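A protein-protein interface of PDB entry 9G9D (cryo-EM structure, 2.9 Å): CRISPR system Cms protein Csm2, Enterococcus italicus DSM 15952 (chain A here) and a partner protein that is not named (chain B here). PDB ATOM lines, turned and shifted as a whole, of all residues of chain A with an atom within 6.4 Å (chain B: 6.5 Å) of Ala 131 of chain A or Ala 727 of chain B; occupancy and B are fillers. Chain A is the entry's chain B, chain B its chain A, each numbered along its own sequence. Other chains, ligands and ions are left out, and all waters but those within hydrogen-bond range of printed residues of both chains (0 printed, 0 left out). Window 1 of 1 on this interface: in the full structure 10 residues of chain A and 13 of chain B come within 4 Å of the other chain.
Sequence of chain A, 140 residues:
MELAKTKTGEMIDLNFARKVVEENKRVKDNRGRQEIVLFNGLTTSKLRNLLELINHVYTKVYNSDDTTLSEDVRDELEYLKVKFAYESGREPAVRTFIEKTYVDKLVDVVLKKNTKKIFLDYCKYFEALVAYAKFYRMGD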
ATOM      1  N   LEU A  14     -20.928 -35.314  -3.231  1.00  0.00           N
ATOM      2  CA  LEU A  14     -20.169 -34.098  -2.953  1.00  0.00           C
ATOM      3  C   LEU A  14     -20.170 -33.168  -4.159  1.00  0.00           C
ATOM      4  O   LEU A  14     -20.160 -31.937  -4.011  1.00  0.00           O
ATOM      5  CB  LEU A  14     -18.744 -34.460  -2.548  1.00  0.00           C
ATOM      6  CG  LEU A  14     -18.636 -35.600  -1.536  1.00  0.00           C
ATOM      7  CD1 LEU A  14     -17.187 -35.973  -1.311  1.00  0.00           C
ATOM      8  CD2 LEU A  14     -19.290 -35.209  -0.229  1.00  0.00           C
ATOM      9  N   LYS A 124     -19.946 -36.796   5.324  1.00  0.00           N
ATOM     10  CA  LYS A 124     -19.093 -36.193   4.305  1.00  0.00           C
ATOM     11  C   LYS A 124     -19.879 -35.214   3.446  1.00  0.00           C
ATOM     12  O   LYS A 124     -19.373 -34.147   3.090  1.00  0.00           O
ATOM     13  CB  LYS A 124     -18.458 -37.275   3.432  1.00  0.00           C
ATOM     14  CG  LYS A 124     -17.508 -38.203   4.167  1.00  0.00           C
ATOM     15  CD  LYS A 124     -16.921 -39.240   3.221  1.00  0.00           C
ATOM     16  CE  LYS A 124     -16.365 -40.435   3.977  1.00  0.00           C
ATOM     17  NZ  LYS A 124     -15.383 -40.032   5.017  1.00  0.00           N
ATOM     18  N   PHE A 126     -22.569 -33.519   4.375  1.00  0.00           N
ATOM     19  CA  PHE A 126     -22.850 -32.329   5.222  1.00  0.00           C
ATOM     20  C   PHE A 126     -21.594 -31.464   5.279  1.00  0.00           C
ATOM     21  O   PHE A 126     -21.685 -30.239   5.059  1.00  0.00           O
ATOM     22  CB  PHE A 126     -23.302 -32.855   6.586  1.00  0.00           C
ATOM     23  CG  PHE A 126     -24.279 -31.968   7.345  1.00  0.00           C
ATOM     24  CD1 PHE A 126     -24.177 -30.582   7.300  1.00  0.00           C
ATOM     25  CD2 PHE A 126     -25.316 -32.527   8.082  1.00  0.00           C
ATOM     26  CE1 PHE A 126     -25.073 -29.783   7.992  1.00  0.00           C
ATOM     27  CE2 PHE A 126     -26.210 -31.723   8.771  1.00  0.00           C
ATOM     28  CZ  PHE A 126     -26.088 -30.355   8.721  1.00  0.00           C
ATOM     29  N   GLU A 127     -20.445 -32.081   5.557  1.00  0.00           N
ATOM     30  CA  GLU A 127     -19.190 -31.349   5.654  1.00  0.00           C
ATOM     31  C   GLU A 127     -18.857 -30.657   4.341  1.00  0.00           C
ATOM     32  O   GLU A 127     -18.340 -29.537   4.337  1.00  0.00           O
ATOM     33  CB  GLU A 127     -18.067 -32.298   6.062  1.00  0.00           C
ATOM     34  CG  GLU A 127     -16.685 -31.684   6.012  1.00  0.00           C
ATOM     35  CD  GLU A 127     -15.593 -32.710   6.217  1.00  0.00           C
ATOM     36  OE1 GLU A 127     -15.925 -33.889   6.460  1.00  0.00           O
ATOM     37  OE2 GLU A 127     -14.405 -32.341   6.133  1.00  0.00           O
ATOM     38  N   ALA A 128     -19.138 -31.314   3.214  1.00  0.00           N
ATOM     39  CA  ALA A 128     -18.916 -30.695   1.914  1.00  0.00           C
ATOM     40  C   ALA A 128     -19.839 -29.504   1.707  1.00  0.00           C
ATOM     41  O   ALA A 128     -19.432 -28.488   1.134  1.00  0.00           O
ATOM     42  CB  ALA A 128     -19.106 -31.726   0.803  1.00  0.00           C
ATOM     43  N   LEU A 129     -21.092 -29.615   2.153  1.00  0.00           N
ATOM     44  CA  LEU A 129     -21.996 -28.470   2.086  1.00  0.00           C
ATOM     45  C   LEU A 129     -21.434 -27.291   2.868  1.00  0.00           C
ATOM     46  O   LEU A 129     -21.405 -26.160   2.369  1.00  0.00           O
ATOM     47  CB  LEU A 129     -23.375 -28.854   2.623  1.00  0.00           C
ATOM     48  CG  LEU A 129     -24.213 -29.859   1.834  1.00  0.00           C
ATOM     49  CD1 LEU A 129     -25.396 -30.314   2.667  1.00  0.00           C
ATOM     50  CD2 LEU A 129     -24.691 -29.245   0.534  1.00  0.00           C
ATOM     51  N   VAL A 130     -20.955 -27.547   4.086  1.00  0.00           N
ATOM     52  CA  VAL A 130     -20.369 -26.480   4.898  1.00  0.00           C
ATOM     53  C   VAL A 130     -19.133 -25.901   4.215  1.00  0.00           C
ATOM     54  O   VAL A 130     -18.949 -24.676   4.159  1.00  0.00           O
ATOM     55  CB  VAL A 130     -20.043 -27.005   6.309  1.00  0.00           C
ATOM     56  CG1 VAL A 130     -19.397 -25.917   7.145  1.00  0.00           C
ATOM     57  CG2 VAL A 130     -21.302 -27.517   6.983  1.00  0.00           C
ATOM     58  N   ALA A 131     -18.271 -26.771   3.685  1.00  0.00           N
ATOM     59  CA  ALA A 131     -17.027 -26.321   3.070  1.00  0.00           C
ATOM     60  C   ALA A 131     -17.290 -25.459   1.844  1.00  0.00           C
ATOM     61  O   ALA A 131     -16.670 -24.404   1.674  1.00  0.00           O
ATOM     62  CB  ALA A 131     -16.165 -27.525   2.702  1.00  0.00           C
ATOM     63  N   TYR A 132     -18.211 -25.886   0.979  1.00  0.00           N
ATOM     64  CA  TYR A 132     -18.494 -25.111  -0.224  1.00  0.00           C
ATOM     65  C   TYR A 132     -19.258 -23.839   0.110  1.00  0.00           C
ATOM     66  O   TYR A 132     -19.118 -22.826  -0.583  1.00  0.00           O
ATOM     67  CB  TYR A 132     -19.258 -25.961  -1.236  1.00  0.00           C
ATOM     68  CG  TYR A 132     -18.408 -27.025  -1.893  1.00  0.00           C
ATOM     69  CD1 TYR A 132     -17.308 -26.681  -2.664  1.00  0.00           C
ATOM     70  CD2 TYR A 132     -18.708 -28.370  -1.748  1.00  0.00           C
ATOM     71  CE1 TYR A 132     -16.530 -27.647  -3.264  1.00  0.00           C
ATOM     72  CE2 TYR A 132     -17.935 -29.342  -2.343  1.00  0.00           C
ATOM     73  CZ  TYR A 132     -16.850 -28.976  -3.101  1.00  0.00           C
ATOM     74  OH  TYR A 132     -16.078 -29.944  -3.699  1.00  0.00           O
ATOM     75  N   ALA A 133     -20.064 -23.860   1.175  1.00  0.00           N
ATOM     76  CA  ALA A 133     -20.692 -22.628   1.631  1.00  0.00           C
ATOM     77  C   ALA A 133     -19.645 -21.621   2.078  1.00  0.00           C
ATOM     78  O   ALA A 133     -19.758 -20.423   1.793  1.00  0.00           O
ATOM     79  CB  ALA A 133     -21.670 -22.929   2.765  1.00  0.00           C
ATOM     80  N   LYS A 134     -18.618 -22.092   2.788  1.00  0.00           N
ATOM     81  CA  LYS A 134     -17.520 -21.214   3.177  1.00  0.00           C
ATOM     82  C   LYS A 134     -16.746 -20.723   1.959  1.00  0.00           C
ATOM     83  O   LYS A 134     -16.344 -19.556   1.897  1.00  0.00           O
ATOM     84  CB  LYS A 134     -16.593 -21.947   4.147  1.00  0.00           C
ATOM     85  CG  LYS A 134     -15.480 -21.097   4.730  1.00  0.00           C
ATOM     86  CD  LYS A 134     -16.034 -19.917   5.508  1.00  0.00           C
ATOM     87  CE  LYS A 134     -15.036 -19.428   6.543  1.00  0.00           C
ATOM     88  NZ  LYS A 134     -13.696 -19.173   5.952  1.00  0.00           N
ATOM     89  N   PHE A 135     -16.530 -21.606   0.981  1.00  0.00           N
ATOM     90  CA  PHE A 135     -15.726 -21.251  -0.185  1.00  0.00           C
ATOM     91  C   PHE A 135     -16.430 -20.221  -1.061  1.00  0.00           C
ATOM     92  O   PHE A 135     -15.797 -19.282  -1.558  1.00  0.00           O
ATOM     93  CB  PHE A 135     -15.395 -22.502  -0.996  1.00  0.00           C
ATOM     94  CG  PHE A 135     -14.604 -22.219  -2.239  1.00  0.00           C
ATOM     95  CD1 PHE A 135     -13.246 -21.961  -2.166  1.00  0.00           C
ATOM     96  CD2 PHE A 135     -15.217 -22.205  -3.479  1.00  0.00           C
ATOM     97  CE1 PHE A 135     -12.515 -21.694  -3.306  1.00  0.00           C
ATOM     98  CE2 PHE A 135     -14.491 -21.940  -4.621  1.00  0.00           C
ATOM     99  CZ  PHE A 135     -13.139 -21.683  -4.533  1.00  0.00           C
ATOM    100  N   TYR A 136     -17.735 -20.376  -1.265  1.00  0.00           N
ATOM    101  CA  TYR A 136     -18.464 -19.506  -2.180  1.00  0.00           C
ATOM    102  C   TYR A 136     -18.883 -18.186  -1.549  1.00  0.00           C
ATOM    103  O   TYR A 136     -19.493 -17.362  -2.235  1.00  0.00           O
ATOM    104  CB  TYR A 136     -19.698 -20.228  -2.729  1.00  0.00           C
ATOM    105  CG  TYR A 136     -19.375 -21.274  -3.772  1.00  0.00           C
ATOM    106  CD1 TYR A 136     -18.772 -20.922  -4.970  1.00  0.00           C
ATOM    107  CD2 TYR A 136     -19.682 -22.610  -3.563  1.00  0.00           C
ATOM    108  CE1 TYR A 136     -18.476 -21.872  -5.925  1.00  0.00           C
ATOM    109  CE2 TYR A 136     -19.390 -23.567  -4.512  1.00  0.00           C
ATOM    110  CZ  TYR A 136     -18.788 -23.193  -5.691  1.00  0.00           C
ATOM    111  OH  TYR A 136     -18.494 -24.142  -6.641  1.00  0.00           O
ATOM    112  N   GLN B 723     -12.888 -37.891  -2.335  1.00  0.00           N
ATOM    113  CA  GLN B 723     -13.266 -36.615  -2.990  1.00  0.00           C
ATOM    114  C   GLN B 723     -13.598 -35.600  -1.894  1.00  0.00           C
ATOM    115  O   GLN B 723     -13.733 -34.399  -2.203  1.00  0.00           O
ATOM    116  CB  GLN B 723     -14.461 -36.803  -3.922  1.00  0.00           C
ATOM    117  CG  GLN B 723     -14.172 -36.420  -5.368  1.00  0.00           C
ATOM    118  CD  GLN B 723     -15.421 -36.147  -6.175  1.00  0.00           C
ATOM    119  OE1 GLN B 723     -16.544 -36.172  -5.658  1.00  0.00           O
ATOM    120  NE2 GLN B 723     -15.233 -35.869  -7.457  1.00  0.00           N
ATOM    121  N   ILE B 724     -13.736 -36.085  -0.660  1.00  0.00           N
ATOM    122  CA  ILE B 724     -14.081 -35.169   0.423  1.00  0.00           C
ATOM    123  C   ILE B 724     -12.960 -34.159   0.636  1.00  0.00           C
ATOM    124  O   ILE B 724     -13.207 -32.994   0.971  1.00  0.00           O
ATOM    125  CB  ILE B 724     -14.398 -35.954   1.710  1.00  0.00           C
ATOM    126  CG1 ILE B 724     -14.767 -34.998   2.845  1.00  0.00           C
ATOM    127  CG2 ILE B 724     -13.225 -36.843   2.105  1.00  0.00           C
ATOM    128  CD1 ILE B 724     -15.966 -34.131   2.539  1.00  0.00           C
ATOM    129  N   ASN B 725     -11.718 -34.595   0.403  1.00  0.00           N
ATOM    130  CA  ASN B 725     -10.544 -33.703   0.617  1.00  0.00           C
ATOM    131  C   ASN B 725     -10.612 -32.538  -0.371  1.00  0.00           C
ATOM    132  O   ASN B 725     -10.064 -31.465  -0.051  1.00  0.00           O
ATOM    133  CB  ASN B 725      -9.235 -34.477   0.539  1.00  0.00           C
ATOM    134  CG  ASN B 725      -9.070 -35.411   1.712  1.00  0.00           C
ATOM    135  OD1 ASN B 725      -9.854 -36.350   1.876  1.00  0.00           O
ATOM    136  ND2 ASN B 725      -8.056 -35.176   2.532  1.00  0.00           N
ATOM    137  N   ILE B 726     -11.252 -32.740  -1.525  1.00  0.00           N
ATOM    138  CA  ILE B 726     -11.426 -31.641  -2.470  1.00  0.00           C
ATOM    139  C   ILE B 726     -12.286 -30.547  -1.852  1.00  0.00           C
ATOM    140  O   ILE B 726     -12.004 -29.352  -2.006  1.00  0.00           O
ATOM    141  CB  ILE B 726     -12.024 -32.158  -3.791  1.00  0.00           C
ATOM    142  CG1 ILE B 726     -11.030 -33.080  -4.497  1.00  0.00           C
ATOM    143  CG2 ILE B 726     -12.413 -31.002  -4.694  1.00  0.00           C
ATOM    144  CD1 ILE B 726     -11.514 -33.580  -5.838  1.00  0.00           C
ATOM    145  N   ALA B 727     -13.345 -30.935  -1.140  1.00  0.00           N
ATOM    146  CA  ALA B 727     -14.136 -29.957  -0.401  1.00  0.00           C
ATOM    147  C   ALA B 727     -13.326 -29.348   0.735  1.00  0.00           C
ATOM    148  O   ALA B 727     -13.403 -28.141   0.985  1.00  0.00           O
ATOM    149  CB  ALA B 727     -15.411 -30.605   0.133  1.00  0.00           C
ATOM    150  N   ARG B 728     -12.544 -30.174   1.436  1.00  0.00           N
ATOM    151  CA  ARG B 728     -11.716 -29.668   2.527  1.00  0.00           C
ATOM    152  C   ARG B 728     -10.674 -28.684   2.016  1.00  0.00           C
ATOM    153  O   ARG B 728     -10.359 -27.696   2.690  1.00  0.00           O
ATOM    154  CB  ARG B 728     -11.045 -30.830   3.258  1.00  0.00           C
ATOM    155  CG  ARG B 728     -12.014 -31.756   3.962  1.00  0.00           C
ATOM    156  CD  ARG B 728     -11.299 -32.962   4.540  1.00  0.00           C
ATOM    157  NE  ARG B 728     -12.224 -33.865   5.212  1.00  0.00           N
ATOM    158  CZ  ARG B 728     -11.901 -35.069   5.664  1.00  0.00           C
ATOM    159  NH1 ARG B 728     -10.680 -35.555   5.524  1.00  0.00           N
ATOM    160  NH2 ARG B 728     -12.828 -35.803   6.271  1.00  0.00           N
ATOM    161  N   LEU B 729     -10.135 -28.956   0.825  1.00  0.00           N
ATOM    162  CA  LEU B 729      -9.161 -28.010   0.223  1.00  0.00           C
ATOM    163  C   LEU B 729      -9.874 -26.668   0.036  1.00  0.00           C
ATOM    164  O   LEU B 729      -9.315 -25.638   0.450  1.00  0.00           O
ATOM    165  CB  LEU B 729      -8.606 -28.516  -1.105  1.00  0.00           C
ATOM    166  CG  LEU B 729      -7.452 -27.690  -1.681  1.00  0.00           C
ATOM    167  CD1 LEU B 729      -6.186 -27.883  -0.865  1.00  0.00           C
ATOM    168  CD2 LEU B 729      -7.205 -27.988  -3.145  1.00  0.00           C
ATOM    169  N   ALA B 730     -11.064 -26.697  -0.565  1.00  0.00           N
ATOM    170  CA  ALA B 730     -11.810 -25.460  -0.759  1.00  0.00           C
ATOM    171  C   ALA B 730     -12.051 -24.760   0.570  1.00  0.00           C
ATOM    172  O   ALA B 730     -11.947 -23.532   0.662  1.00  0.00           O
ATOM    173  CB  ALA B 730     -13.134 -25.747  -1.464  1.00  0.00           C
ATOM    174  N   TYR B 731     -12.375 -25.528   1.612  1.00  0.00           N
ATOM    175  CA  TYR B 731     -12.521 -24.946   2.942  1.00  0.00           C
ATOM    176  C   TYR B 731     -11.204 -24.359   3.429  1.00  0.00           C
ATOM    177  O   TYR B 731     -11.176 -23.258   3.990  1.00  0.00           O
ATOM    178  CB  TYR B 731     -13.035 -26.002   3.920  1.00  0.00           C
ATOM    179  CG  TYR B 731     -13.402 -25.455   5.279  1.00  0.00           C
ATOM    180  CD1 TYR B 731     -14.488 -24.609   5.435  1.00  0.00           C
ATOM    181  CD2 TYR B 731     -12.670 -25.797   6.408  1.00  0.00           C
ATOM    182  CE1 TYR B 731     -14.830 -24.110   6.670  1.00  0.00           C
ATOM    183  CE2 TYR B 731     -13.007 -25.303   7.650  1.00  0.00           C
ATOM    184  CZ  TYR B 731     -14.087 -24.459   7.773  1.00  0.00           C
ATOM    185  OH  TYR B 731     -14.433 -23.959   9.005  1.00  0.00           O
ATOM    186  N   LEU B 732     -10.100 -25.080   3.218  1.00  0.00           N
ATOM    187  CA  LEU B 732      -8.789 -24.569   3.605  1.00  0.00           C
ATOM    188  C   LEU B 732      -8.427 -23.325   2.806  1.00  0.00           C
ATOM    189  O   LEU B 732      -7.863 -22.370   3.351  1.00  0.00           O
ATOM    190  CB  LEU B 732      -7.733 -25.660   3.419  1.00  0.00           C
ATOM    191  CG  LEU B 732      -6.320 -25.426   3.957  1.00  0.00           C
ATOM    192  CD1 LEU B 732      -5.776 -26.715   4.542  1.00  0.00           C
ATOM    193  CD2 LEU B 732      -5.396 -24.926   2.866  1.00  0.00           C
ATOM    194  N   ALA B 734     -10.484 -21.181   1.526  1.00  0.00           N
ATOM    195  CA  ALA B 734     -11.380 -20.068   1.823  1.00  0.00           C
ATOM    196  C   ALA B 734     -10.827 -19.178   2.931  1.00  0.00           C
ATOM    197  O   ALA B 734     -10.864 -17.947   2.823  1.00  0.00           O
ATOM    198  CB  ALA B 734     -12.762 -20.596   2.203  1.00  0.00           C
ATOM    199  N   PHE B 747      -7.893 -24.591  -6.799  1.00  0.00           N
ATOM    200  CA  PHE B 747      -9.091 -25.419  -6.712  1.00  0.00           C
ATOM    201  C   PHE B 747      -9.353 -26.150  -8.024  1.00  0.00           C
ATOM    202  O   PHE B 747      -9.698 -27.336  -8.023  1.00  0.00           O
ATOM    203  CB  PHE B 747     -10.292 -24.556  -6.324  1.00  0.00           C
ATOM    204  CG  PHE B 747     -11.490 -25.345  -5.882  1.00  0.00           C
ATOM    205  CD1 PHE B 747     -11.350 -26.635  -5.401  1.00  0.00           C
ATOM    206  CD2 PHE B 747     -12.758 -24.797  -5.954  1.00  0.00           C
ATOM    207  CE1 PHE B 747     -12.449 -27.359  -4.997  1.00  0.00           C
ATOM    208  CE2 PHE B 747     -13.860 -25.518  -5.551  1.00  0.00           C
ATOM    209  CZ  PHE B 747     -13.705 -26.800  -5.073  1.00  0.00           C
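CD1 of Leu 14 of chain A touches C of Gln 723 of chain B, at 3.7 Å. Ile 724 of chain B touches Leu 14 of chain A. Ile 724 of chain B touches Glu 127 of chain A (CD1 to OE1, 3.9 Å). CB of Ala 128 of chain A touches CB of Ala 727 of chain B, 3.9 Å away. Ala 131 of chain A touches Ala 727 of chain B (CB to O, 3.3 Å). CB of Tyr 731 of chain B touches CB of Ala 131 of chain A, 3.7 Å away. OH of Tyr 132 of chain A touches CG2 of Ile 726 of chain B, at 3.9 Å. Lys 134 of chain A touches Tyr 731 of chain B (CB to CD1, 3.6 Å). Ala 734 of chain B touches Lys 134 of chain A (CB to O, 3.7 Å). O of Ala 730 of chain B touches CD1 of Phe 135 of chain A, at 3.5 Å.
Of the 13 printed residues of chain A, 8 touch a printed residue of chain B. Hydrophobic or aromatic side chains of chain A within 4 Å of the printed part of chain B: Leu 14, Ala 128, Ala 131, Tyr 132 and Phe 135. Along chain A the printed residues that touch a printed residue of chain B span positions 14 to 135.
Val 130 of chain A touches none of the printed residues of chain B. Ala 131 of chain A touches two residues of chain B. Tyr 136 of chain A touches none of the printed residues of chain B. Of the printed residues of chain A, Ile 726 of chain B touches Tyr 132. Of chain A, only Ala 128 (3.9 Å), Ala 131 (3.3 Å) and Tyr 132 (3.8 Å) come within 4 Å of Ala 727 of chain B. Of the printed residues of chain A, Tyr 731 of chain B touches Ala 131 and Lys 134. The nearest residue of chain B that does not touch Ala 131 of chain A is Arg 728 of chain B (4.7 Å). The nearest printed residue of chain A that does not touch Tyr 731 of chain B is Val 130 of chain A (4.6 Å).
The side-chain carboxylate of Glu 127 of chain A lies within salt-bridge range of the guanidinium group of Arg 728 of chain B.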
